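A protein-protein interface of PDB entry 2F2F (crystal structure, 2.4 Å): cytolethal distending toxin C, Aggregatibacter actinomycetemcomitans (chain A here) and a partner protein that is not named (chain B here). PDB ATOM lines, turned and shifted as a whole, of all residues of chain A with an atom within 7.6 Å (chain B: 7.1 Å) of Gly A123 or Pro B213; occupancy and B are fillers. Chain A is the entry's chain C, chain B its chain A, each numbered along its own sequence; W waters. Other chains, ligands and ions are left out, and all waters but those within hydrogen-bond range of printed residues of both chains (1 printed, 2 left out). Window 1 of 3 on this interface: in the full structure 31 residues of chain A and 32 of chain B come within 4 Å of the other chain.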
ATOM      1  N   LEU A  45      -8.612  29.886   1.762  1.00  0.00           N
ATOM      2  CA  LEU A  45      -8.915  28.460   1.703  1.00  0.00           C
ATOM      3  C   LEU A  45      -9.538  28.023   0.373  1.00  0.00           C
ATOM      4  O   LEU A  45      -9.557  26.839   0.035  1.00  0.00           O
ATOM      5  CB  LEU A  45      -9.803  28.057   2.887  1.00  0.00           C
ATOM      6  CG  LEU A  45      -9.067  27.986   4.233  1.00  0.00           C
ATOM      7  CD1 LEU A  45      -9.884  27.154   5.184  1.00  0.00           C
ATOM      8  CD2 LEU A  45      -7.677  27.393   4.079  1.00  0.00           C
ATOM      9  N   ILE A 118     -11.722  36.117  13.347  1.00  0.00           N
ATOM     10  CA  ILE A 118     -12.992  35.585  13.834  1.00  0.00           C
ATOM     11  C   ILE A 118     -12.899  34.069  13.720  1.00  0.00           C
ATOM     12  O   ILE A 118     -12.785  33.524  12.618  1.00  0.00           O
ATOM     13  CB  ILE A 118     -14.163  36.082  12.970  1.00  0.00           C
ATOM     14  CG1 ILE A 118     -14.175  37.616  12.944  1.00  0.00           C
ATOM     15  CG2 ILE A 118     -15.468  35.485  13.469  1.00  0.00           C
ATOM     16  CD1 ILE A 118     -14.930  38.270  14.070  1.00  0.00           C
ATOM     17  N   PRO A 119     -12.994  33.362  14.860  1.00  0.00           N
ATOM     18  CA  PRO A 119     -12.909  31.893  14.894  1.00  0.00           C
ATOM     19  C   PRO A 119     -14.128  31.165  14.311  1.00  0.00           C
ATOM     20  O   PRO A 119     -15.228  31.703  14.288  1.00  0.00           O
ATOM     21  CB  PRO A 119     -12.725  31.597  16.378  1.00  0.00           C
ATOM     22  CG  PRO A 119     -13.445  32.708  17.056  1.00  0.00           C
ATOM     23  CD  PRO A 119     -13.255  33.926  16.195  1.00  0.00           C
ATOM     24  N   THR A 120     -13.918  29.941  13.830  1.00  0.00           N
ATOM     25  CA  THR A 120     -14.991  29.136  13.264  1.00  0.00           C
ATOM     26  C   THR A 120     -14.989  27.732  13.863  1.00  0.00           C
ATOM     27  O   THR A 120     -14.086  27.366  14.611  1.00  0.00           O
ATOM     28  CB  THR A 120     -14.878  28.938  11.730  1.00  0.00           C
ATOM     29  OG1 THR A 120     -13.762  29.643  11.219  1.00  0.00           O
ATOM     30  CG2 THR A 120     -16.046  29.515  11.044  1.00  0.00           C
ATOM     31  N   ASN A 121     -15.997  26.944  13.497  1.00  0.00           N
ATOM     32  CA  ASN A 121     -16.109  25.585  13.981  1.00  0.00           C
ATOM     33  C   ASN A 121     -15.179  24.622  13.252  1.00  0.00           C
ATOM     34  O   ASN A 121     -15.047  23.467  13.649  1.00  0.00           O
ATOM     35  CB  ASN A 121     -17.559  25.110  13.847  1.00  0.00           C
ATOM     36  CG  ASN A 121     -18.011  25.004  12.398  1.00  0.00           C
ATOM     37  OD1 ASN A 121     -17.559  25.759  11.521  1.00  0.00           O
ATOM     38  ND2 ASN A 121     -18.914  24.076  12.141  1.00  0.00           N
ATOM     39  N   THR A 122     -14.515  25.083  12.201  1.00  0.00           N
ATOM     40  CA  THR A 122     -13.609  24.206  11.465  1.00  0.00           C
ATOM     41  C   THR A 122     -12.119  24.485  11.626  1.00  0.00           C
ATOM     42  O   THR A 122     -11.286  23.684  11.197  1.00  0.00           O
ATOM     43  CB  THR A 122     -13.917  24.210   9.960  1.00  0.00           C
ATOM     44  OG1 THR A 122     -13.599  25.493   9.421  1.00  0.00           O
ATOM     45  CG2 THR A 122     -15.398  23.919   9.726  1.00  0.00           C
ATOM     46  N   GLY A 123     -11.762  25.603  12.242  1.00  0.00           N
ATOM     47  CA  GLY A 123     -10.347  25.924  12.376  1.00  0.00           C
ATOM     48  C   GLY A 123      -9.931  26.978  11.355  1.00  0.00           C
ATOM     49  O   GLY A 123      -8.813  27.464  11.383  1.00  0.00           O
ATOM     50  N   ALA A 124     -10.836  27.303  10.436  1.00  0.00           N
ATOM     51  CA  ALA A 124     -10.595  28.317   9.409  1.00  0.00           C
ATOM     52  C   ALA A 124     -10.882  29.635  10.090  1.00  0.00           C
ATOM     53  O   ALA A 124     -11.473  29.651  11.158  1.00  0.00           O
ATOM     54  CB  ALA A 124     -11.557  28.142   8.240  1.00  0.00           C
ATOM     55  N   PHE A 125     -10.456  30.737   9.489  1.00  0.00           N
ATOM     56  CA  PHE A 125     -10.738  32.028  10.087  1.00  0.00           C
ATOM     57  C   PHE A 125     -11.374  32.996   9.113  1.00  0.00           C
ATOM     58  O   PHE A 125     -11.060  32.996   7.924  1.00  0.00           O
ATOM     59  CB  PHE A 125      -9.456  32.655  10.637  1.00  0.00           C
ATOM     60  CG  PHE A 125      -8.981  32.032  11.899  1.00  0.00           C
ATOM     61  CD1 PHE A 125      -9.449  32.484  13.127  1.00  0.00           C
ATOM     62  CD2 PHE A 125      -8.092  30.969  11.867  1.00  0.00           C
ATOM     63  CE1 PHE A 125      -9.034  31.879  14.310  1.00  0.00           C
ATOM     64  CE2 PHE A 125      -7.673  30.358  13.042  1.00  0.00           C
ATOM     65  CZ  PHE A 125      -8.146  30.815  14.264  1.00  0.00           C
ATOM     66  N   LEU A 126     -12.267  33.820   9.637  1.00  0.00           N
ATOM     67  CA  LEU A 126     -12.892  34.857   8.851  1.00  0.00           C
ATOM     68  C   LEU A 126     -12.030  36.034   9.265  1.00  0.00           C
ATOM     69  O   LEU A 126     -11.652  36.134  10.433  1.00  0.00           O
ATOM     70  CB  LEU A 126     -14.323  35.096   9.302  1.00  0.00           C
ATOM     71  CG  LEU A 126     -15.360  34.524   8.342  1.00  0.00           C
ATOM     72  CD1 LEU A 126     -15.404  33.003   8.439  1.00  0.00           C
ATOM     73  CD2 LEU A 126     -16.693  35.138   8.668  1.00  0.00           C
ATOM     74  N   LEU A 160     -15.902  28.888   1.312  1.00  0.00           N
ATOM     75  CA  LEU A 160     -14.451  29.034   1.303  1.00  0.00           C
ATOM     76  C   LEU A 160     -13.937  30.416   0.930  1.00  0.00           C
ATOM     77  O   LEU A 160     -12.842  30.791   1.333  1.00  0.00           O
ATOM     78  CB  LEU A 160     -13.820  27.975   0.403  1.00  0.00           C
ATOM     79  CG  LEU A 160     -13.975  26.539   0.913  1.00  0.00           C
ATOM     80  CD1 LEU A 160     -13.350  25.589  -0.070  1.00  0.00           C
ATOM     81  CD2 LEU A 160     -13.300  26.386   2.255  1.00  0.00           C
ATOM     82  N   GLN A 163     -13.079  32.194   3.934  1.00  0.00           N
ATOM     83  CA  GLN A 163     -12.179  31.512   4.852  1.00  0.00           C
ATOM     84  C   GLN A 163     -10.694  31.613   4.592  1.00  0.00           C
ATOM     85  O   GLN A 163     -10.232  31.509   3.447  1.00  0.00           O
ATOM     86  CB  GLN A 163     -12.586  30.043   4.957  1.00  0.00           C
ATOM     87  CG  GLN A 163     -14.047  29.856   5.346  1.00  0.00           C
ATOM     88  CD  GLN A 163     -14.451  28.405   5.331  1.00  0.00           C
ATOM     89  OE1 GLN A 163     -13.638  27.516   5.628  1.00  0.00           O
ATOM     90  NE2 GLN A 163     -15.710  28.144   4.974  1.00  0.00           N
ATOM     91  N   TRP A 164      -9.953  31.789   5.686  1.00  0.00           N
ATOM     92  CA  TRP A 164      -8.511  31.923   5.640  1.00  0.00           C
ATOM     93  C   TRP A 164      -7.855  30.927   6.561  1.00  0.00           C
ATOM     94  O   TRP A 164      -8.402  30.586   7.598  1.00  0.00           O
ATOM     95  CB  TRP A 164      -8.122  33.341   6.047  1.00  0.00           C
ATOM     96  CG  TRP A 164      -8.681  34.340   5.112  1.00  0.00           C
ATOM     97  CD1 TRP A 164      -9.904  34.923   5.176  1.00  0.00           C
ATOM     98  CD2 TRP A 164      -8.079  34.789   3.895  1.00  0.00           C
ATOM     99  NE1 TRP A 164     -10.114  35.711   4.071  1.00  0.00           N
ATOM    100  CE2 TRP A 164      -9.004  35.642   3.267  1.00  0.00           C
ATOM    101  CE3 TRP A 164      -6.852  34.549   3.279  1.00  0.00           C
ATOM    102  CZ2 TRP A 164      -8.738  36.262   2.043  1.00  0.00           C
ATOM    103  CZ3 TRP A 164      -6.580  35.156   2.068  1.00  0.00           C
ATOM    104  CH2 TRP A 164      -7.519  36.007   1.462  1.00  0.00           C
ATOM    105  N   GLY A 165      -6.690  30.440   6.167  1.00  0.00           N
ATOM    106  CA  GLY A 165      -5.978  29.500   6.999  1.00  0.00           C
ATOM    107  C   GLY A 165      -4.703  30.179   7.451  1.00  0.00           C
ATOM    108  O   GLY A 165      -3.984  30.735   6.622  1.00  0.00           O
ATOM    109  N   ILE A 166      -4.442  30.171   8.756  1.00  0.00           N
ATOM    110  CA  ILE A 166      -3.216  30.745   9.320  1.00  0.00           C
ATOM    111  C   ILE A 166      -2.296  29.539   9.439  1.00  0.00           C
ATOM    112  O   ILE A 166      -2.362  28.777  10.406  1.00  0.00           O
ATOM    113  CB  ILE A 166      -3.493  31.382  10.701  1.00  0.00           C
ATOM    114  CG1 ILE A 166      -4.475  32.542  10.522  1.00  0.00           C
ATOM    115  CG2 ILE A 166      -2.203  31.870  11.328  1.00  0.00           C
ATOM    116  CD1 ILE A 166      -4.808  33.259  11.772  1.00  0.00           C
ATOM    117  N   LEU A 167      -1.448  29.364   8.428  1.00  0.00           N
ATOM    118  CA  LEU A 167      -0.587  28.194   8.353  1.00  0.00           C
ATOM    119  C   LEU A 167       0.920  28.420   8.429  1.00  0.00           C
ATOM    120  O   LEU A 167       1.384  29.544   8.455  1.00  0.00           O
ATOM    121  CB  LEU A 167      -0.948  27.420   7.064  1.00  0.00           C
ATOM    122  CG  LEU A 167      -2.455  27.153   6.869  1.00  0.00           C
ATOM    123  CD1 LEU A 167      -2.778  26.981   5.401  1.00  0.00           C
ATOM    124  CD2 LEU A 167      -2.865  25.908   7.636  1.00  0.00           C
ATOM    125  N   PRO B  73     -18.031  18.823  12.023  1.00  0.00           N
ATOM    126  CA  PRO B  73     -17.042  19.461  11.138  1.00  0.00           C
ATOM    127  C   PRO B  73     -15.654  19.590  11.760  1.00  0.00           C
ATOM    128  O   PRO B  73     -14.646  19.296  11.114  1.00  0.00           O
ATOM    129  CB  PRO B  73     -17.655  20.826  10.850  1.00  0.00           C
ATOM    130  CG  PRO B  73     -19.089  20.630  10.999  1.00  0.00           C
ATOM    131  CD  PRO B  73     -19.279  19.605  12.072  1.00  0.00           C
ATOM    132  N   SER B  74     -15.617  20.005  13.027  1.00  0.00           N
ATOM    133  CA  SER B  74     -14.362  20.174  13.750  1.00  0.00           C
ATOM    134  C   SER B  74     -13.539  18.904  13.749  1.00  0.00           C
ATOM    135  O   SER B  74     -12.351  18.922  14.056  1.00  0.00           O
ATOM    136  CB  SER B  74     -14.641  20.583  15.192  1.00  0.00           C
ATOM    137  OG  SER B  74     -15.386  19.582  15.871  1.00  0.00           O
ATOM    138  N   PHE B  76     -12.888  17.146  11.107  1.00  0.00           N
ATOM    139  CA  PHE B  76     -12.210  16.946   9.835  1.00  0.00           C
ATOM    140  C   PHE B  76     -11.259  18.074   9.459  1.00  0.00           C
ATOM    141  O   PHE B  76     -11.424  19.222   9.873  1.00  0.00           O
ATOM    142  CB  PHE B  76     -13.237  16.717   8.718  1.00  0.00           C
ATOM    143  CG  PHE B  76     -14.267  15.675   9.059  1.00  0.00           C
ATOM    144  CD1 PHE B  76     -13.977  14.329   8.919  1.00  0.00           C
ATOM    145  CD2 PHE B  76     -15.502  16.042   9.597  1.00  0.00           C
ATOM    146  CE1 PHE B  76     -14.893  13.351   9.316  1.00  0.00           C
ATOM    147  CE2 PHE B  76     -16.417  15.086   9.995  1.00  0.00           C
ATOM    148  CZ  PHE B  76     -16.114  13.732   9.855  1.00  0.00           C
ATOM    149  N   MET B  77     -10.284  17.726   8.635  1.00  0.00           N
ATOM    150  CA  MET B  77      -9.261  18.650   8.179  1.00  0.00           C
ATOM    151  C   MET B  77      -8.760  18.246   6.799  1.00  0.00           C
ATOM    152  O   MET B  77      -9.233  17.279   6.217  1.00  0.00           O
ATOM    153  CB  MET B  77      -8.071  18.625   9.136  1.00  0.00           C
ATOM    154  CG  MET B  77      -7.572  17.238   9.448  1.00  0.00           C
ATOM    155  SD  MET B  77      -6.432  16.552   8.263  1.00  0.00           S
ATOM    156  CE  MET B  77      -4.903  17.130   8.864  1.00  0.00           C
ATOM    157  N   THR B  78      -7.826  19.020   6.258  1.00  0.00           N
ATOM    158  CA  THR B  78      -7.245  18.687   4.972  1.00  0.00           C
ATOM    159  C   THR B  78      -5.750  18.675   5.159  1.00  0.00           C
ATOM    160  O   THR B  78      -5.243  19.410   5.991  1.00  0.00           O
ATOM    161  CB  THR B  78      -7.599  19.721   3.892  1.00  0.00           C
ATOM    162  OG1 THR B  78      -7.337  21.043   4.383  1.00  0.00           O
ATOM    163  CG2 THR B  78      -9.068  19.588   3.491  1.00  0.00           C
ATOM    164  N   LEU B  79      -5.052  17.825   4.414  1.00  0.00           N
ATOM    165  CA  LEU B  79      -3.605  17.778   4.460  1.00  0.00           C
ATOM    166  C   LEU B  79      -3.203  18.545   3.186  1.00  0.00           C
ATOM    167  O   LEU B  79      -3.260  18.001   2.085  1.00  0.00           O
ATOM    168  CB  LEU B  79      -3.131  16.331   4.395  1.00  0.00           C
ATOM    169  CG  LEU B  79      -3.139  15.612   5.739  1.00  0.00           C
ATOM    170  CD1 LEU B  79      -3.179  14.100   5.507  1.00  0.00           C
ATOM    171  CD2 LEU B  79      -1.895  16.022   6.547  1.00  0.00           C
ATOM    172  N   MET B  80      -2.786  19.801   3.361  1.00  0.00           N
ATOM    173  CA  MET B  80      -2.429  20.701   2.268  1.00  0.00           C
ATOM    174  C   MET B  80      -0.940  20.777   1.987  1.00  0.00           C
ATOM    175  O   MET B  80      -0.151  21.025   2.885  1.00  0.00           O
ATOM    176  CB  MET B  80      -2.933  22.104   2.602  1.00  0.00           C
ATOM    177  CG  MET B  80      -2.630  23.150   1.539  1.00  0.00           C
ATOM    178  SD  MET B  80      -3.124  24.826   1.966  1.00  0.00           S
ATOM    179  CE  MET B  80      -4.866  24.652   2.421  1.00  0.00           C
ATOM    180  N   LEU B  86      -4.491  19.469  -1.810  1.00  0.00           N
ATOM    181  CA  LEU B  86      -5.038  18.615  -0.742  1.00  0.00           C
ATOM    182  C   LEU B  86      -4.983  17.114  -1.043  1.00  0.00           C
ATOM    183  O   LEU B  86      -5.472  16.674  -2.074  1.00  0.00           O
ATOM    184  CB  LEU B  86      -6.491  19.002  -0.505  1.00  0.00           C
ATOM    185  CG  LEU B  86      -6.815  20.486  -0.610  1.00  0.00           C
ATOM    186  CD1 LEU B  86      -8.309  20.748  -0.499  1.00  0.00           C
ATOM    187  CD2 LEU B  86      -6.093  21.196   0.493  1.00  0.00           C
ATOM    188  N   ASN B 114     -11.703  15.566   2.649  1.00  0.00           N
ATOM    189  CA  ASN B 114     -11.552  15.822   4.079  1.00  0.00           C
ATOM    190  C   ASN B 114     -11.255  14.520   4.819  1.00  0.00           C
ATOM    191  O   ASN B 114     -11.776  13.468   4.462  1.00  0.00           O
ATOM    192  CB  ASN B 114     -12.824  16.467   4.619  1.00  0.00           C
ATOM    193  CG  ASN B 114     -13.038  17.847   4.051  1.00  0.00           C
ATOM    194  OD1 ASN B 114     -12.081  18.575   3.813  1.00  0.00           O
ATOM    195  ND2 ASN B 114     -14.291  18.222   3.834  1.00  0.00           N
ATOM    196  N   TYR B 210       0.640  20.790   5.437  1.00  0.00           N
ATOM    197  CA  TYR B 210       0.113  21.642   6.474  1.00  0.00           C
ATOM    198  C   TYR B 210      -1.159  20.974   6.973  1.00  0.00           C
ATOM    199  O   TYR B 210      -1.927  20.427   6.182  1.00  0.00           O
ATOM    200  CB  TYR B 210      -0.224  23.038   5.916  1.00  0.00           C
ATOM    201  CG  TYR B 210       0.855  23.678   5.045  1.00  0.00           C
ATOM    202  CD1 TYR B 210       2.209  23.582   5.373  1.00  0.00           C
ATOM    203  CD2 TYR B 210       0.508  24.402   3.895  1.00  0.00           C
ATOM    204  CE1 TYR B 210       3.191  24.190   4.584  1.00  0.00           C
ATOM    205  CE2 TYR B 210       1.480  25.013   3.099  1.00  0.00           C
ATOM    206  CZ  TYR B 210       2.818  24.905   3.448  1.00  0.00           C
ATOM    207  OH  TYR B 210       3.772  25.530   2.679  1.00  0.00           O
ATOM    208  N   LEU B 211      -1.351  20.979   8.288  1.00  0.00           N
ATOM    209  CA  LEU B 211      -2.554  20.433   8.896  1.00  0.00           C
ATOM    210  C   LEU B 211      -3.463  21.646   8.828  1.00  0.00           C
ATOM    211  O   LEU B 211      -3.324  22.569   9.618  1.00  0.00           O
ATOM    212  CB  LEU B 211      -2.282  20.034  10.344  1.00  0.00           C
ATOM    213  CG  LEU B 211      -1.119  19.057  10.497  1.00  0.00           C
ATOM    214  CD1 LEU B 211      -0.789  18.888  11.965  1.00  0.00           C
ATOM    215  CD2 LEU B 211      -1.476  17.707   9.883  1.00  0.00           C
ATOM    216  N   ALA B 212      -4.401  21.637   7.892  1.00  0.00           N
ATOM    217  CA  ALA B 212      -5.272  22.793   7.692  1.00  0.00           C
ATOM    218  C   ALA B 212      -6.745  22.493   7.845  1.00  0.00           C
ATOM    219  O   ALA B 212      -7.142  21.338   7.992  1.00  0.00           O
ATOM    220  CB  ALA B 212      -5.021  23.381   6.299  1.00  0.00           C
ATOM    221  N   PRO B 213      -7.575  23.549   7.837  1.00  0.00           N
ATOM    222  CA  PRO B 213      -9.018  23.366   7.973  1.00  0.00           C
ATOM    223  C   PRO B 213      -9.564  22.490   6.845  1.00  0.00           C
ATOM    224  O   PRO B 213      -8.982  22.411   5.765  1.00  0.00           O
ATOM    225  CB  PRO B 213      -9.559  24.793   7.905  1.00  0.00           C
ATOM    226  CG  PRO B 213      -8.422  25.648   8.327  1.00  0.00           C
ATOM    227  CD  PRO B 213      -7.217  24.977   7.773  1.00  0.00           C
ATOM    228  N   PRO B 214     -10.694  21.811   7.097  1.00  0.00           N
ATOM    229  CA  PRO B 214     -11.263  20.955   6.057  1.00  0.00           C
ATOM    230  C   PRO B 214     -11.868  21.848   5.009  1.00  0.00           C
ATOM    231  O   PRO B 214     -12.036  23.041   5.250  1.00  0.00           O
ATOM    232  CB  PRO B 214     -12.332  20.173   6.798  1.00  0.00           C
ATOM    233  CG  PRO B 214     -12.801  21.113   7.829  1.00  0.00           C
ATOM    234  CD  PRO B 214     -11.535  21.808   8.306  1.00  0.00           C
ATOM    235  N   VAL B 215     -12.168  21.296   3.837  1.00  0.00           N
ATOM    236  CA  VAL B 215     -12.822  22.116   2.830  1.00  0.00           C
ATOM    237  C   VAL B 215     -14.316  21.877   3.071  1.00  0.00           C
ATOM    238  O   VAL B 215     -14.903  20.914   2.584  1.00  0.00           O
ATOM    239  CB  VAL B 215     -12.400  21.738   1.377  1.00  0.00           C
ATOM    240  CG1 VAL B 215     -11.142  22.526   0.984  1.00  0.00           C
ATOM    241  CG2 VAL B 215     -12.130  20.260   1.276  1.00  0.00           C
ATOM    242  N   LEU B 216     -14.902  22.759   3.881  1.00  0.00           N
ATOM    243  CA  LEU B 216     -16.309  22.716   4.270  1.00  0.00           C
ATOM    244  C   LEU B 216     -16.726  24.149   4.561  1.00  0.00           C
ATOM    245  O   LEU B 216     -15.879  25.040   4.683  1.00  0.00           O
ATOM    246  CB  LEU B 216     -16.501  21.917   5.569  1.00  0.00           C
ATOM    247  CG  LEU B 216     -16.155  20.433   5.659  1.00  0.00           C
ATOM    248  CD1 LEU B 216     -16.041  20.011   7.117  1.00  0.00           C
ATOM    249  CD2 LEU B 216     -17.246  19.637   4.980  1.00  0.00           C
ATOM    250  N   ALA B 218     -17.884  27.007   6.928  1.00  0.00           N
ATOM    251  CA  ALA B 218     -17.522  27.237   8.315  1.00  0.00           C
ATOM    252  C   ALA B 218     -18.497  28.156   8.976  1.00  0.00           C
ATOM    253  O   ALA B 218     -18.986  29.085   8.359  1.00  0.00           O
ATOM    254  CB  ALA B 218     -16.131  27.829   8.385  1.00  0.00           C
HETATM  255  O   HOH W   1     -17.449  21.382  14.671  1.00  0.00           O
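The side-chain amide nitrogen of Gln A163 sits at hydrogen-bond distance from the backbone carbonyl oxygen of Leu B216.
N of Ala B218 sits close to NE2 of Gln A163 (3.1 Å).
The backbone NH (N) of Thr B78 lies within hydrogen-bond range of the backbone carbonyl oxygen (O) of Ala B212, 3.0 Å away.
OG1 of Thr B78 lies within hydrogen-bond range of O of Pro B213, at 2.5 Å.
The side-chain amide oxygen (OD1) of Asn B114 sits at hydrogen-bond distance from the backbone NH (N) of Val B215 (2.7 Å).
N of Leu A45 is in hydrogen-bond range of O of Gln A163 (2.8 Å).
The side-chain hydroxyl (OG1) of Thr A122 sits close to the backbone NH (N) of Ala A124.
Among the printed residues, pairs that only touch across the chains: Leu A45 with Pro B213 (3.6 Å), Thr A120 with Ala B218 (3.1 Å), Asn A121 with Pro B73 (3.6 Å), Asn A121 with Ser B74 (3.3 Å), Asn A121 with Ala B218 (3.5 Å), Thr A122 with Pro B73 (3.99 Å), Thr A122 with Pro B213 (3.9 Å), Thr A122 with Pro B214 (3.5 Å), Thr A122 with Ala B218 (3.6 Å), Gly A123 with Pro B213 (3.6 Å), Ala A124 with Pro B213 (3.6 Å), Leu A160 with Val B215 (3.9 Å), Leu A160 with Leu B216 (3.8 Å), Leu A167 with Leu B211 (3.9 Å) and Leu A167 with Ala B212 (3.6 Å).
Of chain B, only Pro B213 comes within 4 Å of Gly A123.
Of chain A, only Leu A45, Thr A122, Gly A123 and Ala A124 come within 4 Å of Pro B213.
Of the printed residues of chain B, Asn A121 touches Pro B73, Ser B74 and Ala B218.
Printed residues of chain B within 4 Å of Leu A45: Pro B213 (3.6 Å).
Of the printed residues of chain A, Pro B73 touches Asn A121 and Thr A122.
Met B80 touches none of the printed residues of chain A.
Met B77 touches none of the printed residues of chain A.
The nearest residue of chain B that does not touch Gly A123 is Pro B214 (5.5 Å).
The nearest printed residue of chain A that does not touch Pro B73 is Gly A123 (7.0 Å).
Of the 17 printed residues of chain B, 9 touch a printed residue of chain A.
Printed residues of chain B that touch a printed residue of chain A: Pro B73, Ser B74, Leu B211, Ala B212, Pro B213, Pro B214, Val B215, Leu B216 and Ala B218.
Among the printed residues, no Asp or Glu carboxylate lies within 4 Å of a Lys or Arg side-chain nitrogen of the other chain.
Water W1 lies within hydrogen-bond range of the backbone NH (N) of Ser B74 (2.8 Å) and the backbone carbonyl oxygen (O) of Asn A121 (3.3 Å).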
